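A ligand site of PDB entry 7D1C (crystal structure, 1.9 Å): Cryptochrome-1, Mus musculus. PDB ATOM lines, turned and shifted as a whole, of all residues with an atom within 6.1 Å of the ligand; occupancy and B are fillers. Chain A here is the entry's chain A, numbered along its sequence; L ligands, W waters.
Residues that only touch the ligand: Trp 294 (3.4 Å), Arg 295 (3.4 Å), Phe 298 (3.8 Å), His 357 (3.2 Å), His 361 (3.9 Å), Ala 364 (3.6 Å), Phe 383 (3.2 Å), Asp 389 (3.3 Å), Ala 390 (3.8 Å), Ile 394 (3.3 Å), Asn 395 (3.5 Å), Trp 401 (3.3 Å), Leu 402 (3.5 Å) and Phe 411 (3.9 Å).
Hydrophobic or aromatic side chains that line the ligand: Trp 294, Phe 298, His 357, His 361, Ala 364, Phe 383, Ala 390, Ile 394, Trp 399, Trp 401, Leu 402 and Phe 411.
Within 4 Å of the ligand: Gln 291, Trp 294, Arg 295, Phe 298, His 357, Arg 360, His 361, Ala 364, Phe 383, Asp 389, Ala 390, Ile 394, Asn 395, Ser 398, Trp 399, Trp 401, Leu 402 and Phe 411.
The nearest printed residue that does not touch the ligand is Leu 387 (4.02 Å).
The guanidinium group (NH1) of Arg 360 sits at hydrogen-bond distance from a nitrogen (N2) of the ligand, at 3.0 Å.
NE2 of Gln 291 lies close to O1 of the ligand.
The indole nitrogen of Trp 399 lies within hydrogen-bond range of an oxygen (O2) of the ligand, at 3.2 Å.
OG of Ser 398 lies within hydrogen-bond range of N1 of the ligand, at 2.9 Å.
The guanidinium group of Arg 295 lies within hydrogen-bond range of the backbone carbonyl oxygen of Leu 257 (3.1 Å).
The guanidinium group (NH2) of Arg 360 lies within salt-bridge range of the side-chain carboxylate (OD2) of Asp 389 (2.8 Å).
OD2 of Asp 389 sits at hydrogen-bond distance from OG of Ser 254 (2.7 Å).
The indole nitrogen (NE1) of Trp 399 lies close to the side-chain amide oxygen (OD1) of Asn 395 (3.3 Å).
OG of Ser 398 lies within hydrogen-bond range of O of Ile 394, at 2.8 Å.
Water W1 lies within hydrogen-bond range of ND1 of His 357 and NE2 of His 361.
Water W2 lies within hydrogen-bond range of NE2 of His 357 (2.6 Å) and OD2 of Asp 389 (2.7 Å).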
ATOM      1  N   SER A 254      12.027 -31.483  24.114  1.00  0.00           N
ATOM      2  CA  SER A 254      11.313 -31.542  22.844  1.00  0.00           C
ATOM      3  C   SER A 254      12.224 -31.679  21.623  1.00  0.00           C
ATOM      4  O   SER A 254      11.892 -32.460  20.718  1.00  0.00           O
ATOM      5  CB  SER A 254      10.362 -30.335  22.688  1.00  0.00           C
ATOM      6  OG  SER A 254      11.057 -29.096  22.692  1.00  0.00           O
ATOM      7  N   LEU A 257      13.345 -35.418  21.326  1.00  0.00           N
ATOM      8  CA  LEU A 257      12.330 -36.315  20.785  1.00  0.00           C
ATOM      9  C   LEU A 257      12.200 -36.166  19.276  1.00  0.00           C
ATOM     10  O   LEU A 257      11.903 -37.150  18.583  1.00  0.00           O
ATOM     11  CB  LEU A 257      10.981 -36.040  21.456  1.00  0.00           C
ATOM     12  CG  LEU A 257      10.902 -36.384  22.945  1.00  0.00           C
ATOM     13  CD1 LEU A 257       9.734 -35.653  23.608  1.00  0.00           C
ATOM     14  CD2 LEU A 257      10.779 -37.891  23.141  1.00  0.00           C
ATOM     15  N   GLN A 291       2.619 -33.352  25.451  1.00  0.00           N
ATOM     16  CA  GLN A 291       2.564 -33.225  23.995  1.00  0.00           C
ATOM     17  C   GLN A 291       2.734 -34.549  23.270  1.00  0.00           C
ATOM     18  O   GLN A 291       2.629 -34.573  22.045  1.00  0.00           O
ATOM     19  CB  GLN A 291       3.632 -32.236  23.526  1.00  0.00           C
ATOM     20  CG  GLN A 291       3.124 -30.832  23.228  1.00  0.00           C
ATOM     21  CD  GLN A 291       2.185 -30.294  24.281  1.00  0.00           C
ATOM     22  OE1 GLN A 291       2.456 -30.375  25.484  1.00  0.00           O
ATOM     23  NE2 GLN A 291       1.065 -29.722  23.838  1.00  0.00           N
ATOM     24  N   LEU A 292       2.992 -35.643  23.993  1.00  0.00           N
ATOM     25  CA  LEU A 292       3.350 -36.909  23.358  1.00  0.00           C
ATOM     26  C   LEU A 292       2.251 -37.424  22.440  1.00  0.00           C
ATOM     27  O   LEU A 292       2.522 -38.021  21.393  1.00  0.00           O
ATOM     28  CB  LEU A 292       3.688 -37.955  24.413  1.00  0.00           C
ATOM     29  CG  LEU A 292       5.107 -37.968  24.961  1.00  0.00           C
ATOM     30  CD1 LEU A 292       5.418 -39.319  25.578  1.00  0.00           C
ATOM     31  CD2 LEU A 292       6.108 -37.628  23.865  1.00  0.00           C
ATOM     32  N   TRP A 294      -0.362 -35.421  21.174  1.00  0.00           N
ATOM     33  CA  TRP A 294      -0.422 -34.463  20.087  1.00  0.00           C
ATOM     34  C   TRP A 294       0.607 -34.805  19.019  1.00  0.00           C
ATOM     35  O   TRP A 294       0.295 -34.837  17.824  1.00  0.00           O
ATOM     36  CB  TRP A 294      -0.185 -33.045  20.614  1.00  0.00           C
ATOM     37  CG  TRP A 294      -1.410 -32.444  21.180  1.00  0.00           C
ATOM     38  CD1 TRP A 294      -1.680 -32.210  22.498  1.00  0.00           C
ATOM     39  CD2 TRP A 294      -2.550 -31.986  20.452  1.00  0.00           C
ATOM     40  NE1 TRP A 294      -2.917 -31.643  22.630  1.00  0.00           N
ATOM     41  CE2 TRP A 294      -3.473 -31.488  21.384  1.00  0.00           C
ATOM     42  CE3 TRP A 294      -2.875 -31.953  19.088  1.00  0.00           C
ATOM     43  CZ2 TRP A 294      -4.709 -30.963  21.006  1.00  0.00           C
ATOM     44  CZ3 TRP A 294      -4.098 -31.424  18.714  1.00  0.00           C
ATOM     45  CH2 TRP A 294      -5.002 -30.932  19.672  1.00  0.00           C
ATOM     46  N   ARG A 295       1.841 -35.072  19.448  1.00  0.00           N
ATOM     47  CA  ARG A 295       2.880 -35.561  18.551  1.00  0.00           C
ATOM     48  C   ARG A 295       2.388 -36.770  17.753  1.00  0.00           C
ATOM     49  O   ARG A 295       2.447 -36.785  16.523  1.00  0.00           O
ATOM     50  CB  ARG A 295       4.105 -35.924  19.390  1.00  0.00           C
ATOM     51  CG  ARG A 295       5.350 -36.319  18.625  1.00  0.00           C
ATOM     52  CD  ARG A 295       6.474 -36.631  19.608  1.00  0.00           C
ATOM     53  NE  ARG A 295       7.706 -37.047  18.949  1.00  0.00           N
ATOM     54  CZ  ARG A 295       8.036 -38.311  18.730  1.00  0.00           C
ATOM     55  NH1 ARG A 295       7.226 -39.291  19.115  1.00  0.00           N
ATOM     56  NH2 ARG A 295       9.187 -38.602  18.121  1.00  0.00           N
ATOM     57  N   PHE A 298      -0.483 -35.912  15.130  1.00  0.00           N
ATOM     58  CA  PHE A 298      -0.132 -35.270  13.875  1.00  0.00           C
ATOM     59  C   PHE A 298       0.637 -36.207  12.942  1.00  0.00           C
ATOM     60  O   PHE A 298       0.447 -36.158  11.721  1.00  0.00           O
ATOM     61  CB  PHE A 298       0.671 -33.999  14.138  1.00  0.00           C
ATOM     62  CG  PHE A 298      -0.168 -32.852  14.654  1.00  0.00           C
ATOM     63  CD1 PHE A 298      -1.289 -32.430  13.944  1.00  0.00           C
ATOM     64  CD2 PHE A 298       0.146 -32.213  15.841  1.00  0.00           C
ATOM     65  CE1 PHE A 298      -2.070 -31.384  14.420  1.00  0.00           C
ATOM     66  CE2 PHE A 298      -0.636 -31.166  16.317  1.00  0.00           C
ATOM     67  CZ  PHE A 298      -1.746 -30.752  15.602  1.00  0.00           C
ATOM     68  N   TYR A 299       1.496 -37.076  13.495  1.00  0.00           N
ATOM     69  CA  TYR A 299       2.120 -38.098  12.663  1.00  0.00           C
ATOM     70  C   TYR A 299       1.062 -38.977  12.004  1.00  0.00           C
ATOM     71  O   TYR A 299       1.184 -39.315  10.814  1.00  0.00           O
ATOM     72  CB  TYR A 299       3.075 -38.958  13.486  1.00  0.00           C
ATOM     73  CG  TYR A 299       4.402 -38.310  13.801  1.00  0.00           C
ATOM     74  CD1 TYR A 299       5.169 -37.725  12.804  1.00  0.00           C
ATOM     75  CD2 TYR A 299       4.891 -38.284  15.104  1.00  0.00           C
ATOM     76  CE1 TYR A 299       6.396 -37.133  13.094  1.00  0.00           C
ATOM     77  CE2 TYR A 299       6.104 -37.705  15.405  1.00  0.00           C
ATOM     78  CZ  TYR A 299       6.853 -37.125  14.395  1.00  0.00           C
ATOM     79  OH  TYR A 299       8.057 -36.548  14.701  1.00  0.00           O
ATOM     80  N   HIS A 357       5.303 -23.034  23.793  1.00  0.00           N
ATOM     81  CA  HIS A 357       4.147 -23.355  22.969  1.00  0.00           C
ATOM     82  C   HIS A 357       3.153 -22.197  22.918  1.00  0.00           C
ATOM     83  O   HIS A 357       2.580 -21.918  21.861  1.00  0.00           O
ATOM     84  CB  HIS A 357       3.473 -24.618  23.486  1.00  0.00           C
ATOM     85  CG  HIS A 357       3.896 -25.860  22.774  1.00  0.00           C
ATOM     86  ND1 HIS A 357       3.046 -26.609  21.993  1.00  0.00           N
ATOM     87  CD2 HIS A 357       5.113 -26.472  22.707  1.00  0.00           C
ATOM     88  CE1 HIS A 357       3.704 -27.635  21.482  1.00  0.00           C
ATOM     89  NE2 HIS A 357       4.956 -27.578  21.905  1.00  0.00           N
ATOM     90  N   ARG A 360       4.358 -19.758  20.553  1.00  0.00           N
ATOM     91  CA  ARG A 360       4.014 -20.213  19.213  1.00  0.00           C
ATOM     92  C   ARG A 360       2.592 -19.815  18.837  1.00  0.00           C
ATOM     93  O   ARG A 360       2.349 -19.313  17.735  1.00  0.00           O
ATOM     94  CB  ARG A 360       4.179 -21.730  19.098  1.00  0.00           C
ATOM     95  CG  ARG A 360       5.614 -22.201  19.256  1.00  0.00           C
ATOM     96  CD  ARG A 360       5.755 -23.729  19.368  1.00  0.00           C
ATOM     97  NE  ARG A 360       6.961 -24.067  20.108  1.00  0.00           N
ATOM     98  CZ  ARG A 360       7.665 -25.187  19.961  1.00  0.00           C
ATOM     99  NH1 ARG A 360       7.283 -26.113  19.097  1.00  0.00           N
ATOM    100  NH2 ARG A 360       8.758 -25.368  20.695  1.00  0.00           N
ATOM    101  N   HIS A 361       1.626 -20.028  19.750  1.00  0.00           N
ATOM    102  CA  HIS A 361       0.254 -19.595  19.504  1.00  0.00           C
ATOM    103  C   HIS A 361       0.193 -18.103  19.220  1.00  0.00           C
ATOM    104  O   HIS A 361      -0.526 -17.661  18.315  1.00  0.00           O
ATOM    105  CB  HIS A 361      -0.629 -19.924  20.715  1.00  0.00           C
ATOM    106  CG  HIS A 361      -0.885 -21.382  20.910  1.00  0.00           C
ATOM    107  ND1 HIS A 361      -2.048 -21.856  21.490  1.00  0.00           N
ATOM    108  CD2 HIS A 361      -0.145 -22.475  20.620  1.00  0.00           C
ATOM    109  CE1 HIS A 361      -2.004 -23.172  21.543  1.00  0.00           C
ATOM    110  NE2 HIS A 361      -0.860 -23.576  21.016  1.00  0.00           N
ATOM    111  N   VAL A 363       2.527 -15.930  17.980  1.00  0.00           N
ATOM    112  CA  VAL A 363       3.051 -15.452  16.710  1.00  0.00           C
ATOM    113  C   VAL A 363       2.301 -16.073  15.543  1.00  0.00           C
ATOM    114  O   VAL A 363       2.242 -15.485  14.459  1.00  0.00           O
ATOM    115  CB  VAL A 363       4.570 -15.703  16.604  1.00  0.00           C
ATOM    116  CG1 VAL A 363       5.310 -14.952  17.707  1.00  0.00           C
ATOM    117  CG2 VAL A 363       4.886 -17.189  16.665  1.00  0.00           C
ATOM    118  N   ALA A 364       1.717 -17.260  15.735  1.00  0.00           N
ATOM    119  CA  ALA A 364       0.915 -17.870  14.680  1.00  0.00           C
ATOM    120  C   ALA A 364      -0.385 -17.110  14.477  1.00  0.00           C
ATOM    121  O   ALA A 364      -0.809 -16.869  13.338  1.00  0.00           O
ATOM    122  CB  ALA A 364       0.625 -19.333  14.990  1.00  0.00           C
ATOM    123  N   PHE A 383       8.985 -21.652  10.477  1.00  0.00           N
ATOM    124  CA  PHE A 383       9.196 -22.542  11.616  1.00  0.00           C
ATOM    125  C   PHE A 383      10.003 -23.765  11.214  1.00  0.00           C
ATOM    126  O   PHE A 383      10.867 -24.218  11.963  1.00  0.00           O
ATOM    127  CB  PHE A 383       7.851 -22.946  12.221  1.00  0.00           C
ATOM    128  CG  PHE A 383       7.355 -22.002  13.284  1.00  0.00           C
ATOM    129  CD1 PHE A 383       7.621 -20.642  13.205  1.00  0.00           C
ATOM    130  CD2 PHE A 383       6.631 -22.481  14.368  1.00  0.00           C
ATOM    131  CE1 PHE A 383       7.159 -19.774  14.179  1.00  0.00           C
ATOM    132  CE2 PHE A 383       6.168 -21.614  15.342  1.00  0.00           C
ATOM    133  CZ  PHE A 383       6.440 -20.263  15.249  1.00  0.00           C
ATOM    134  N   LEU A 387      12.847 -24.024  13.800  1.00  0.00           N
ATOM    135  CA  LEU A 387      12.360 -24.700  14.999  1.00  0.00           C
ATOM    136  C   LEU A 387      12.988 -26.078  15.116  1.00  0.00           C
ATOM    137  O   LEU A 387      12.974 -26.856  14.163  1.00  0.00           O
ATOM    138  CB  LEU A 387      10.832 -24.814  14.960  1.00  0.00           C
ATOM    139  CG  LEU A 387      10.091 -25.252  16.223  1.00  0.00           C
ATOM    140  CD1 LEU A 387      10.453 -24.354  17.409  1.00  0.00           C
ATOM    141  CD2 LEU A 387       8.591 -25.221  15.955  1.00  0.00           C
ATOM    142  N   ASP A 389      12.169 -28.604  17.279  1.00  0.00           N
ATOM    143  CA  ASP A 389      11.424 -29.718  17.871  1.00  0.00           C
ATOM    144  C   ASP A 389      10.169 -30.122  17.108  1.00  0.00           C
ATOM    145  O   ASP A 389       9.375 -30.910  17.627  1.00  0.00           O
ATOM    146  CB  ASP A 389      11.074 -29.387  19.326  1.00  0.00           C
ATOM    147  CG  ASP A 389      10.011 -28.294  19.467  1.00  0.00           C
ATOM    148  OD1 ASP A 389       9.519 -27.757  18.460  1.00  0.00           O
ATOM    149  OD2 ASP A 389       9.670 -27.978  20.626  1.00  0.00           O
ATOM    150  N   ALA A 390       9.963 -29.625  15.891  1.00  0.00           N
ATOM    151  CA  ALA A 390       8.737 -29.929  15.153  1.00  0.00           C
ATOM    152  C   ALA A 390       9.073 -30.497  13.781  1.00  0.00           C
ATOM    153  O   ALA A 390       9.691 -29.821  12.962  1.00  0.00           O
ATOM    154  CB  ALA A 390       7.857 -28.684  15.008  1.00  0.00           C
ATOM    155  N   ASP A 391       8.653 -31.737  13.544  1.00  0.00           N
ATOM    156  CA  ASP A 391       8.788 -32.383  12.246  1.00  0.00           C
ATOM    157  C   ASP A 391       7.828 -31.765  11.231  1.00  0.00           C
ATOM    158  O   ASP A 391       6.945 -30.962  11.573  1.00  0.00           O
ATOM    159  CB  ASP A 391       8.508 -33.879  12.368  1.00  0.00           C
ATOM    160  CG  ASP A 391       9.746 -34.694  12.664  1.00  0.00           C
ATOM    161  OD1 ASP A 391      10.855 -34.249  12.273  1.00  0.00           O
ATOM    162  OD2 ASP A 391       9.627 -35.779  13.267  1.00  0.00           O
ATOM    163  N   ILE A 394       4.271 -32.427  12.320  1.00  0.00           N
ATOM    164  CA  ILE A 394       3.808 -31.679  13.479  1.00  0.00           C
ATOM    165  C   ILE A 394       3.722 -30.194  13.153  1.00  0.00           C
ATOM    166  O   ILE A 394       2.761 -29.512  13.537  1.00  0.00           O
ATOM    167  CB  ILE A 394       4.717 -31.954  14.689  1.00  0.00           C
ATOM    168  CG1 ILE A 394       4.290 -33.245  15.416  1.00  0.00           C
ATOM    169  CG2 ILE A 394       4.689 -30.796  15.675  1.00  0.00           C
ATOM    170  CD1 ILE A 394       4.422 -34.519  14.612  1.00  0.00           C
ATOM    171  N   ASN A 395       4.708 -29.674  12.423  1.00  0.00           N
ATOM    172  CA  ASN A 395       4.682 -28.280  12.006  1.00  0.00           C
ATOM    173  C   ASN A 395       3.453 -27.980  11.157  1.00  0.00           C
ATOM    174  O   ASN A 395       2.695 -27.046  11.438  1.00  0.00           O
ATOM    175  CB  ASN A 395       5.969 -27.944  11.247  1.00  0.00           C
ATOM    176  CG  ASN A 395       6.314 -26.470  11.278  1.00  0.00           C
ATOM    177  OD1 ASN A 395       5.870 -25.734  12.157  1.00  0.00           O
ATOM    178  ND2 ASN A 395       7.115 -26.031  10.319  1.00  0.00           N
ATOM    179  N   GLY A 397       0.590 -29.713  10.782  1.00  0.00           N
ATOM    180  CA  GLY A 397      -0.653 -29.852  11.529  1.00  0.00           C
ATOM    181  C   GLY A 397      -0.873 -28.740  12.518  1.00  0.00           C
ATOM    182  O   GLY A 397      -1.995 -28.226  12.662  1.00  0.00           O
ATOM    183  N   SER A 398       0.190 -28.311  13.214  1.00  0.00           N
ATOM    184  CA  SER A 398       0.045 -27.273  14.219  1.00  0.00           C
ATOM    185  C   SER A 398      -0.360 -25.945  13.579  1.00  0.00           C
ATOM    186  O   SER A 398      -1.202 -25.221  14.109  1.00  0.00           O
ATOM    187  CB  SER A 398       1.353 -27.102  15.001  1.00  0.00           C
ATOM    188  OG  SER A 398       1.643 -28.270  15.764  1.00  0.00           O
ATOM    189  N   TRP A 399       0.234 -25.623  12.422  1.00  0.00           N
ATOM    190  CA  TRP A 399      -0.086 -24.368  11.756  1.00  0.00           C
ATOM    191  C   TRP A 399      -1.500 -24.384  11.187  1.00  0.00           C
ATOM    192  O   TRP A 399      -2.181 -23.356  11.184  1.00  0.00           O
ATOM    193  CB  TRP A 399       0.946 -24.092  10.665  1.00  0.00           C
ATOM    194  CG  TRP A 399       2.122 -23.351  11.195  1.00  0.00           C
ATOM    195  CD1 TRP A 399       3.309 -23.878  11.590  1.00  0.00           C
ATOM    196  CD2 TRP A 399       2.208 -21.935  11.424  1.00  0.00           C
ATOM    197  NE1 TRP A 399       4.144 -22.882  12.033  1.00  0.00           N
ATOM    198  CE2 TRP A 399       3.493 -21.684  11.948  1.00  0.00           C
ATOM    199  CE3 TRP A 399       1.333 -20.866  11.223  1.00  0.00           C
ATOM    200  CZ2 TRP A 399       3.924 -20.398  12.277  1.00  0.00           C
ATOM    201  CZ3 TRP A 399       1.758 -19.592  11.557  1.00  0.00           C
ATOM    202  CH2 TRP A 399       3.050 -19.369  12.082  1.00  0.00           C
ATOM    203  N   TRP A 401      -4.096 -26.198  12.486  1.00  0.00           N
ATOM    204  CA  TRP A 401      -5.022 -26.149  13.613  1.00  0.00           C
ATOM    205  C   TRP A 401      -5.090 -24.741  14.205  1.00  0.00           C
ATOM    206  O   TRP A 401      -6.177 -24.227  14.480  1.00  0.00           O
ATOM    207  CB  TRP A 401      -4.598 -27.174  14.661  1.00  0.00           C
ATOM    208  CG  TRP A 401      -5.391 -28.449  14.603  1.00  0.00           C
ATOM    209  CD1 TRP A 401      -6.218 -28.945  15.575  1.00  0.00           C
ATOM    210  CD2 TRP A 401      -5.437 -29.391  13.520  1.00  0.00           C
ATOM    211  NE1 TRP A 401      -6.774 -30.130  15.163  1.00  0.00           N
ATOM    212  CE2 TRP A 401      -6.316 -30.429  13.909  1.00  0.00           C
ATOM    213  CE3 TRP A 401      -4.827 -29.458  12.267  1.00  0.00           C
ATOM    214  CZ2 TRP A 401      -6.584 -31.522  13.088  1.00  0.00           C
ATOM    215  CZ3 TRP A 401      -5.093 -30.540  11.454  1.00  0.00           C
ATOM    216  CH2 TRP A 401      -5.975 -31.557  11.864  1.00  0.00           C
ATOM    217  N   LEU A 402      -3.941 -24.108  14.405  1.00  0.00           N
ATOM    218  CA  LEU A 402      -3.920 -22.821  15.094  1.00  0.00           C
ATOM    219  C   LEU A 402      -4.412 -21.674  14.230  1.00  0.00           C
ATOM    220  O   LEU A 402      -4.825 -20.639  14.771  1.00  0.00           O
ATOM    221  CB  LEU A 402      -2.518 -22.540  15.625  1.00  0.00           C
ATOM    222  CG  LEU A 402      -2.095 -23.523  16.725  1.00  0.00           C
ATOM    223  CD1 LEU A 402      -0.651 -23.308  17.126  1.00  0.00           C
ATOM    224  CD2 LEU A 402      -3.022 -23.401  17.934  1.00  0.00           C
ATOM    225  N   GLN A 409     -11.810 -27.503  14.652  1.00  0.00           N
ATOM    226  CA  GLN A 409     -11.082 -26.798  15.700  1.00  0.00           C
ATOM    227  C   GLN A 409     -11.139 -25.316  15.381  1.00  0.00           C
ATOM    228  O   GLN A 409     -10.535 -24.874  14.398  1.00  0.00           O
ATOM    229  CB  GLN A 409      -9.644 -27.280  15.822  1.00  0.00           C
ATOM    230  N   PHE A 411     -10.912 -21.200  16.942  1.00  0.00           N
ATOM    231  CA  PHE A 411     -10.466 -20.285  17.981  1.00  0.00           C
ATOM    232  C   PHE A 411     -11.111 -18.924  17.736  1.00  0.00           C
ATOM    233  O   PHE A 411     -10.921 -18.327  16.667  1.00  0.00           O
ATOM    234  CB  PHE A 411      -8.940 -20.151  18.006  1.00  0.00           C
ATOM    235  CG  PHE A 411      -8.224 -21.431  18.336  1.00  0.00           C
ATOM    236  CD1 PHE A 411      -7.934 -21.762  19.652  1.00  0.00           C
ATOM    237  CD2 PHE A 411      -7.836 -22.308  17.337  1.00  0.00           C
ATOM    238  CE1 PHE A 411      -7.278 -22.934  19.964  1.00  0.00           C
ATOM    239  CE2 PHE A 411      -7.182 -23.490  17.641  1.00  0.00           C
ATOM    240  CZ  PHE A 411      -6.897 -23.802  18.956  1.00  0.00           C
HETATM  241  C1  LIG L   1       4.823 -26.605  16.104  1.00  0.00           C
HETATM  242  C2  LIG L   1       3.687 -24.468  15.856  1.00  0.00           C
HETATM  243  C3  LIG L   1       2.356 -22.493  15.527  1.00  0.00           C
HETATM  244  C4  LIG L   1      -0.235 -28.672  19.326  1.00  0.00           C
HETATM  245  C5  LIG L   1      -2.482 -28.444  20.254  1.00  0.00           C
HETATM  246  C6  LIG L   1      -4.375 -27.290  19.233  1.00  0.00           C
HETATM  247  C7  LIG L   1      -4.529 -26.132  21.490  1.00  0.00           C
HETATM  248  C8  LIG L   1       1.183 -29.088  19.401  1.00  0.00           C
HETATM  249  C9  LIG L   1       3.580 -29.092  18.582  1.00  0.00           C
HETATM  250  C10 LIG L   1       4.336 -30.100  19.148  1.00  0.00           C
HETATM  251  C11 LIG L   1       4.205 -31.401  19.866  1.00  0.00           C
HETATM  252  C12 LIG L   1       6.670 -30.812  19.482  1.00  0.00           C
HETATM  253  C13 LIG L   1       5.724 -29.788  18.944  1.00  0.00           C
HETATM  254  C14 LIG L   1       4.227 -26.885  17.349  1.00  0.00           C
HETATM  255  C15 LIG L   1       4.576 -25.426  15.372  1.00  0.00           C
HETATM  256  C16 LIG L   1       3.047 -24.707  17.084  1.00  0.00           C
HETATM  257  C17 LIG L   1       3.316 -25.901  17.806  1.00  0.00           C
HETATM  258  C18 LIG L   1      -1.162 -28.894  20.334  1.00  0.00           C
HETATM  259  C19 LIG L   1      -2.959 -27.721  19.147  1.00  0.00           C
HETATM  260  C20 LIG L   1      -5.120 -26.927  20.493  1.00  0.00           C
HETATM  261  C21 LIG L   1      -5.178 -25.788  22.685  1.00  0.00           C
HETATM  262  C22 LIG L   1      -6.487 -26.234  22.912  1.00  0.00           C
HETATM  263  C23 LIG L   1      -7.106 -27.035  21.945  1.00  0.00           C
HETATM  264  C24 LIG L   1      -6.430 -27.372  20.756  1.00  0.00           C
HETATM  265  C25 LIG L   1      -2.023 -27.456  18.150  1.00  0.00           C
HETATM  266  C26 LIG L   1      -0.695 -27.914  18.239  1.00  0.00           C
HETATM  267  N1  LIG L   1       2.216 -28.838  18.513  1.00  0.00           N
HETATM  268  N2  LIG L   1       5.834 -28.594  18.268  1.00  0.00           N
HETATM  269  N3  LIG L   1       4.497 -28.141  18.068  1.00  0.00           N
HETATM  270  O1  LIG L   1       1.529 -29.710  20.451  1.00  0.00           O
HETATM  271  O2  LIG L   1       3.442 -23.299  15.125  1.00  0.00           O
HETATM  272  O3  LIG L   1       5.725 -32.971  18.406  1.00  0.00           O
HETATM  273  O4  LIG L   1       6.037 -32.983  20.807  1.00  0.00           O
HETATM  274  O5  LIG L   1      -4.992 -27.199  18.115  1.00  0.00           O
HETATM  275  S1  LIG L   1       5.700 -32.248  19.639  1.00  0.00           S
HETATM  276  O   HOH W   1       0.569 -26.174  21.391  1.00  0.00           O
HETATM  277  O   HOH W   2       7.345 -28.491  21.947  1.00  0.00           O
HETATM  278  O   HOH W   3       9.304 -32.815  20.054  1.00  0.00           O
